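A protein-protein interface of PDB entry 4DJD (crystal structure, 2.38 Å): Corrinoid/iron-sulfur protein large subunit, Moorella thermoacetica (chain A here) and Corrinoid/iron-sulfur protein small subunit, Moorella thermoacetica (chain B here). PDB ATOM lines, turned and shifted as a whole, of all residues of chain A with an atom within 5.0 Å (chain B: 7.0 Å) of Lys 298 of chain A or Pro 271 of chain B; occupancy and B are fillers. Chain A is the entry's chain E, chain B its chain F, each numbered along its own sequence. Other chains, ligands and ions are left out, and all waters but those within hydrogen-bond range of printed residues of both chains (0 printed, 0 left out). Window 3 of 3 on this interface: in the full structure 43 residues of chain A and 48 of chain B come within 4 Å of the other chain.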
ATOM      1  N   GLY A 116      -6.002  19.003  27.205  1.00  0.00           N
ATOM      2  CA  GLY A 116      -7.403  18.948  27.582  1.00  0.00           C
ATOM      3  C   GLY A 116      -7.837  17.563  28.024  1.00  0.00           C
ATOM      4  O   GLY A 116      -8.989  17.360  28.411  1.00  0.00           O
ATOM      5  N   LEU A 117      -6.913  16.608  27.972  1.00  0.00           N
ATOM      6  CA  LEU A 117      -7.216  15.230  28.346  1.00  0.00           C
ATOM      7  C   LEU A 117      -7.250  15.033  29.861  1.00  0.00           C
ATOM      8  O   LEU A 117      -6.478  14.258  30.421  1.00  0.00           O
ATOM      9  CB  LEU A 117      -6.233  14.253  27.691  1.00  0.00           C
ATOM     10  CG  LEU A 117      -6.375  14.070  26.175  1.00  0.00           C
ATOM     11  CD1 LEU A 117      -5.258  13.193  25.622  1.00  0.00           C
ATOM     12  CD2 LEU A 117      -7.738  13.480  25.813  1.00  0.00           C
ATOM     13  N   PHE A 119     -10.428  14.709  33.072  1.00  0.00           N
ATOM     14  CA  PHE A 119     -11.849  14.391  33.148  1.00  0.00           C
ATOM     15  C   PHE A 119     -12.394  14.474  34.563  1.00  0.00           C
ATOM     16  O   PHE A 119     -11.691  14.197  35.531  1.00  0.00           O
ATOM     17  CB  PHE A 119     -12.110  12.984  32.599  1.00  0.00           C
ATOM     18  CG  PHE A 119     -11.484  12.726  31.260  1.00  0.00           C
ATOM     19  CD1 PHE A 119     -10.175  12.277  31.166  1.00  0.00           C
ATOM     20  CD2 PHE A 119     -12.201  12.924  30.097  1.00  0.00           C
ATOM     21  CE1 PHE A 119      -9.598  12.038  29.937  1.00  0.00           C
ATOM     22  CE2 PHE A 119     -11.627  12.689  28.863  1.00  0.00           C
ATOM     23  CZ  PHE A 119     -10.324  12.246  28.782  1.00  0.00           C
ATOM     24  N   ASP A 296      -5.683  10.346  20.996  1.00  0.00           N
ATOM     25  CA  ASP A 296      -5.831  11.469  21.918  1.00  0.00           C
ATOM     26  C   ASP A 296      -7.272  11.972  22.044  1.00  0.00           C
ATOM     27  O   ASP A 296      -7.499  13.103  22.465  1.00  0.00           O
ATOM     28  CB  ASP A 296      -4.899  12.625  21.533  1.00  0.00           C
ATOM     29  CG  ASP A 296      -5.143  13.140  20.119  1.00  0.00           C
ATOM     30  OD1 ASP A 296      -6.104  12.686  19.458  1.00  0.00           O
ATOM     31  OD2 ASP A 296      -4.365  14.011  19.670  1.00  0.00           O
ATOM     32  N   ALA A 297      -8.239  11.131  21.686  1.00  0.00           N
ATOM     33  CA  ALA A 297      -9.646  11.511  21.779  1.00  0.00           C
ATOM     34  C   ALA A 297     -10.188  11.322  23.195  1.00  0.00           C
ATOM     35  O   ALA A 297      -9.846  10.349  23.873  1.00  0.00           O
ATOM     36  CB  ALA A 297     -10.483  10.720  20.777  1.00  0.00           C
ATOM     37  N   LYS A 298     -11.028  12.259  23.634  1.00  0.00           N
ATOM     38  CA  LYS A 298     -11.635  12.193  24.961  1.00  0.00           C
ATOM     39  C   LYS A 298     -12.472  10.925  25.122  1.00  0.00           C
ATOM     40  O   LYS A 298     -12.533  10.348  26.205  1.00  0.00           O
ATOM     41  CB  LYS A 298     -12.519  13.419  25.221  1.00  0.00           C
ATOM     42  CG  LYS A 298     -11.805  14.764  25.197  1.00  0.00           C
ATOM     43  CD  LYS A 298     -12.820  15.900  25.314  1.00  0.00           C
ATOM     44  CE  LYS A 298     -12.161  17.277  25.307  1.00  0.00           C
ATOM     45  NZ  LYS A 298     -11.283  17.500  26.486  1.00  0.00           N
ATOM     46  N   GLU A 299     -13.113  10.503  24.037  1.00  0.00           N
ATOM     47  CA  GLU A 299     -13.976   9.322  24.037  1.00  0.00           C
ATOM     48  C   GLU A 299     -13.198   8.066  24.375  1.00  0.00           C
ATOM     49  O   GLU A 299     -13.759   7.105  24.887  1.00  0.00           O
ATOM     50  CB  GLU A 299     -14.599   9.102  22.657  1.00  0.00           C
ATOM     51  CG  GLU A 299     -15.154  10.322  22.017  1.00  0.00           C
ATOM     52  CD  GLU A 299     -14.141  11.116  21.230  1.00  0.00           C
ATOM     53  OE1 GLU A 299     -13.897  10.766  20.058  1.00  0.00           O
ATOM     54  OE2 GLU A 299     -13.606  12.103  21.778  1.00  0.00           O
ATOM     55  N   HIS A 300     -11.914   8.070  24.042  1.00  0.00           N
ATOM     56  CA  HIS A 300     -11.073   6.891  24.205  1.00  0.00           C
ATOM     57  C   HIS A 300     -10.378   6.887  25.554  1.00  0.00           C
ATOM     58  O   HIS A 300     -10.254   5.843  26.194  1.00  0.00           O
ATOM     59  CB  HIS A 300     -10.031   6.822  23.085  1.00  0.00           C
ATOM     60  CG  HIS A 300     -10.628   6.802  21.714  1.00  0.00           C
ATOM     61  ND1 HIS A 300      -9.903   7.102  20.580  1.00  0.00           N
ATOM     62  CD2 HIS A 300     -11.884   6.517  21.292  1.00  0.00           C
ATOM     63  CE1 HIS A 300     -10.687   7.008  19.522  1.00  0.00           C
ATOM     64  NE2 HIS A 300     -11.893   6.653  19.925  1.00  0.00           N
ATOM     65  N   LEU A 301      -9.921   8.057  25.982  1.00  0.00           N
ATOM     66  CA  LEU A 301      -9.180   8.160  27.229  1.00  0.00           C
ATOM     67  C   LEU A 301     -10.056   7.928  28.456  1.00  0.00           C
ATOM     68  O   LEU A 301      -9.645   7.239  29.388  1.00  0.00           O
ATOM     69  CB  LEU A 301      -8.447   9.500  27.329  1.00  0.00           C
ATOM     70  CG  LEU A 301      -6.986   9.505  26.864  1.00  0.00           C
ATOM     71  CD1 LEU A 301      -6.141   8.581  27.739  1.00  0.00           C
ATOM     72  CD2 LEU A 301      -6.860   9.118  25.399  1.00  0.00           C
ATOM     73  N   LEU A 302     -11.262   8.494  28.449  1.00  0.00           N
ATOM     74  CA  LEU A 302     -12.154   8.402  29.611  1.00  0.00           C
ATOM     75  C   LEU A 302     -12.417   6.972  30.127  1.00  0.00           C
ATOM     76  O   LEU A 302     -12.290   6.728  31.327  1.00  0.00           O
ATOM     77  CB  LEU A 302     -13.468   9.168  29.380  1.00  0.00           C
ATOM     78  CG  LEU A 302     -14.511   9.026  30.495  1.00  0.00           C
ATOM     79  CD1 LEU A 302     -13.992   9.608  31.802  1.00  0.00           C
ATOM     80  CD2 LEU A 302     -15.834   9.670  30.109  1.00  0.00           C
ATOM     81  N   PRO A 303     -12.778   6.026  29.234  1.00  0.00           N
ATOM     82  CA  PRO A 303     -12.937   4.639  29.692  1.00  0.00           C
ATOM     83  C   PRO A 303     -11.644   4.009  30.232  1.00  0.00           C
ATOM     84  O   PRO A 303     -11.692   3.265  31.217  1.00  0.00           O
ATOM     85  CB  PRO A 303     -13.382   3.908  28.420  1.00  0.00           C
ATOM     86  CG  PRO A 303     -14.076   4.952  27.630  1.00  0.00           C
ATOM     87  CD  PRO A 303     -13.264   6.188  27.852  1.00  0.00           C
ATOM     88  N   PRO B 266     -24.894  12.548  25.806  1.00  0.00           N
ATOM     89  CA  PRO B 266     -24.371  13.207  24.606  1.00  0.00           C
ATOM     90  C   PRO B 266     -23.297  14.244  24.922  1.00  0.00           C
ATOM     91  O   PRO B 266     -23.301  14.825  26.008  1.00  0.00           O
ATOM     92  CB  PRO B 266     -25.613  13.873  24.003  1.00  0.00           C
ATOM     93  CG  PRO B 266     -26.598  14.010  25.142  1.00  0.00           C
ATOM     94  CD  PRO B 266     -26.110  13.205  26.318  1.00  0.00           C
ATOM     95  N   VAL B 267     -22.388  14.466  23.977  1.00  0.00           N
ATOM     96  CA  VAL B 267     -21.298  15.418  24.158  1.00  0.00           C
ATOM     97  C   VAL B 267     -21.791  16.861  24.367  1.00  0.00           C
ATOM     98  O   VAL B 267     -21.086  17.683  24.947  1.00  0.00           O
ATOM     99  CB  VAL B 267     -20.287  15.349  22.984  1.00  0.00           C
ATOM    100  CG1 VAL B 267     -20.849  16.026  21.732  1.00  0.00           C
ATOM    101  CG2 VAL B 267     -18.946  15.967  23.385  1.00  0.00           C
ATOM    102  N   SER B 268     -23.001  17.164  23.909  1.00  0.00           N
ATOM    103  CA  SER B 268     -23.564  18.497  24.110  1.00  0.00           C
ATOM    104  C   SER B 268     -23.711  18.820  25.599  1.00  0.00           C
ATOM    105  O   SER B 268     -23.528  19.963  26.014  1.00  0.00           O
ATOM    106  CB  SER B 268     -24.909  18.641  23.392  1.00  0.00           C
ATOM    107  OG  SER B 268     -25.867  17.724  23.895  1.00  0.00           O
ATOM    108  N   GLU B 269     -24.021  17.801  26.397  1.00  0.00           N
ATOM    109  CA  GLU B 269     -24.208  17.977  27.834  1.00  0.00           C
ATOM    110  C   GLU B 269     -22.937  17.690  28.640  1.00  0.00           C
ATOM    111  O   GLU B 269     -22.741  18.250  29.723  1.00  0.00           O
ATOM    112  CB  GLU B 269     -25.366  17.104  28.327  1.00  0.00           C
ATOM    113  CG  GLU B 269     -26.666  17.342  27.569  1.00  0.00           C
ATOM    114  CD  GLU B 269     -27.842  16.579  28.148  1.00  0.00           C
ATOM    115  OE1 GLU B 269     -27.674  15.940  29.210  1.00  0.00           O
ATOM    116  OE2 GLU B 269     -28.935  16.620  27.541  1.00  0.00           O
ATOM    117  N   TYR B 270     -22.077  16.824  28.108  1.00  0.00           N
ATOM    118  CA  TYR B 270     -20.815  16.492  28.769  1.00  0.00           C
ATOM    119  C   TYR B 270     -19.641  16.588  27.801  1.00  0.00           C
ATOM    120  O   TYR B 270     -19.066  15.567  27.422  1.00  0.00           O
ATOM    121  CB  TYR B 270     -20.874  15.084  29.365  1.00  0.00           C
ATOM    122  CG  TYR B 270     -21.929  14.919  30.433  1.00  0.00           C
ATOM    123  CD1 TYR B 270     -23.242  14.617  30.097  1.00  0.00           C
ATOM    124  CD2 TYR B 270     -21.613  15.065  31.775  1.00  0.00           C
ATOM    125  CE1 TYR B 270     -24.210  14.466  31.066  1.00  0.00           C
ATOM    126  CE2 TYR B 270     -22.573  14.916  32.751  1.00  0.00           C
ATOM    127  CZ  TYR B 270     -23.872  14.617  32.391  1.00  0.00           C
ATOM    128  OH  TYR B 270     -24.835  14.466  33.360  1.00  0.00           O
ATOM    129  N   PRO B 271     -19.273  17.820  27.408  1.00  0.00           N
ATOM    130  CA  PRO B 271     -18.238  18.010  26.382  1.00  0.00           C
ATOM    131  C   PRO B 271     -16.899  17.393  26.771  1.00  0.00           C
ATOM    132  O   PRO B 271     -16.114  17.033  25.891  1.00  0.00           O
ATOM    133  CB  PRO B 271     -18.128  19.539  26.262  1.00  0.00           C
ATOM    134  CG  PRO B 271     -18.732  20.082  27.524  1.00  0.00           C
ATOM    135  CD  PRO B 271     -19.792  19.100  27.923  1.00  0.00           C
ATOM    136  N   GLY B 272     -16.653  17.262  28.071  1.00  0.00           N
ATOM    137  CA  GLY B 272     -15.422  16.675  28.563  1.00  0.00           C
ATOM    138  C   GLY B 272     -15.340  15.169  28.368  1.00  0.00           C
ATOM    139  O   GLY B 272     -14.247  14.596  28.353  1.00  0.00           O
ATOM    140  N   TRP B 273     -16.493  14.522  28.214  1.00  0.00           N
ATOM    141  CA  TRP B 273     -16.534  13.072  28.015  1.00  0.00           C
ATOM    142  C   TRP B 273     -16.349  12.673  26.551  1.00  0.00           C
ATOM    143  O   TRP B 273     -16.253  11.487  26.232  1.00  0.00           O
ATOM    144  CB  TRP B 273     -17.838  12.482  28.556  1.00  0.00           C
ATOM    145  CG  TRP B 273     -17.965  12.548  30.054  1.00  0.00           C
ATOM    146  CD1 TRP B 273     -17.046  13.040  30.938  1.00  0.00           C
ATOM    147  CD2 TRP B 273     -19.077  12.102  30.839  1.00  0.00           C
ATOM    148  NE1 TRP B 273     -17.517  12.927  32.224  1.00  0.00           N
ATOM    149  CE2 TRP B 273     -18.763  12.355  32.192  1.00  0.00           C
ATOM    150  CE3 TRP B 273     -20.311  11.519  30.532  1.00  0.00           C
ATOM    151  CZ2 TRP B 273     -19.637  12.048  33.235  1.00  0.00           C
ATOM    152  CZ3 TRP B 273     -21.179  11.211  31.569  1.00  0.00           C
ATOM    153  CH2 TRP B 273     -20.838  11.477  32.906  1.00  0.00           C
ATOM    154  N   GLY B 274     -16.307  13.667  25.665  1.00  0.00           N
ATOM    155  CA  GLY B 274     -16.118  13.423  24.245  1.00  0.00           C
ATOM    156  C   GLY B 274     -17.322  12.792  23.564  1.00  0.00           C
ATOM    157  O   GLY B 274     -18.348  12.551  24.202  1.00  0.00           O
ATOM    158  N   LYS B 275     -17.187  12.532  22.265  1.00  0.00           N
ATOM    159  CA  LYS B 275     -18.255  11.968  21.435  1.00  0.00           C
ATOM    160  C   LYS B 275     -18.866  10.693  22.013  1.00  0.00           C
ATOM    161  O   LYS B 275     -18.153   9.785  22.430  1.00  0.00           O
ATOM    162  CB  LYS B 275     -17.742  11.705  20.018  1.00  0.00           C
ATOM    163  CG  LYS B 275     -17.189  12.943  19.337  1.00  0.00           C
ATOM    164  CD  LYS B 275     -16.773  12.664  17.902  1.00  0.00           C
ATOM    165  CE  LYS B 275     -16.045  13.864  17.311  1.00  0.00           C
ATOM    166  NZ  LYS B 275     -15.649  13.646  15.891  1.00  0.00           N
ATOM    167  N   ARG B 279     -17.567   6.362  22.805  1.00  0.00           N
ATOM    168  CA  ARG B 279     -17.487   6.337  24.260  1.00  0.00           C
ATOM    169  C   ARG B 279     -18.340   5.199  24.821  1.00  0.00           C
ATOM    170  O   ARG B 279     -17.900   4.458  25.692  1.00  0.00           O
ATOM    171  CB  ARG B 279     -17.910   7.678  24.866  1.00  0.00           C
ATOM    172  CG  ARG B 279     -18.217   7.603  26.356  1.00  0.00           C
ATOM    173  CD  ARG B 279     -18.120   8.962  27.037  1.00  0.00           C
ATOM    174  NE  ARG B 279     -18.733  10.038  26.262  1.00  0.00           N
ATOM    175  CZ  ARG B 279     -20.006  10.408  26.362  1.00  0.00           C
ATOM    176  NH1 ARG B 279     -20.819   9.780  27.198  1.00  0.00           N
ATOM    177  NH2 ARG B 279     -20.472  11.401  25.617  1.00  0.00           N
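Hydrophobic or aromatic side chains of chain A that line the printed part of chain B: Phe 119 and Leu 302.
Printed residues of chain B that touch a printed residue of chain A: Pro 271, Gly 272, Trp 273, Gly 274, Lys 275 and Arg 279.
Hydrophobic or aromatic side chains of chain B within 4 Å of the printed part of chain A: Trp 273.
Among the printed residues, 11 pairs touch across the chains.
O of Gly 116 of chain A sits at hydrogen-bond distance from NZ of Lys 298 of chain A, at 3.0 Å.
O of Trp 273 of chain B sits at hydrogen-bond distance from NE of Arg 279 of chain B, 2.9 Å away.
The backbone carbonyl oxygen of Gly 274 of chain B is in hydrogen-bond range of the guanidinium group of Arg 279 of chain B (2.8 Å).
Gly 272 of chain B touches Phe 119 of chain A.
CD of Lys 298 of chain A touches O of Gly 272 of chain B, at 3.6 Å.
O of Trp 273 of chain B touches O of Lys 298 of chain A, at 3.9 Å.
Lys 298 of chain A touches Gly 274 of chain B (CB to CA, 3.7 Å).
Glu 299 of chain A touches Trp 273 of chain B.
Gly 274 of chain B touches Glu 299 of chain A.
Lys 275 of chain B touches Glu 299 of chain A (N to CG, 3.0 Å).
O of Glu 299 of chain A touches CA of Arg 279 of chain B, at 3.9 Å.
Trp 273 of chain B touches Leu 302 of chain A (CG to CD2, 3.6 Å).
CD2 of Leu 302 of chain A touches CD of Arg 279 of chain B, 3.9 Å away.
Of the printed residues of chain B, Phe 119 of chain A touches Gly 272.
Of chain B, only Pro 271 (3.5 Å), Gly 272 (3.6 Å), Trp 273 (3.9 Å) and Gly 274 (3.7 Å) come within 4 Å of Lys 298 of chain A.
Leu 301 of chain A touches none of the printed residues of chain B.
Val 267 of chain B touches none of the printed residues of chain A.
Pro 271 of chain B touches just one residue of chain A: Lys 298 (3.5 Å).
Of the printed residues of chain A, Trp 273 of chain B touches Lys 298 (3.9 Å), Glu 299 (3.8 Å) and Leu 302 (3.6 Å).
Of the printed residues of chain A, Arg 279 of chain B touches Glu 299 and Leu 302.
The nearest residue of chain B that does not touch Lys 298 of chain A is Lys 275 of chain B (5.6 Å).
The nearest printed residue of chain A that does not touch Pro 271 of chain B is Glu 299 of chain A (6.9 Å).
The nearest printed residue of chain B that does not touch Glu 299 of chain A is Gly 272 of chain B (6.1 Å).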
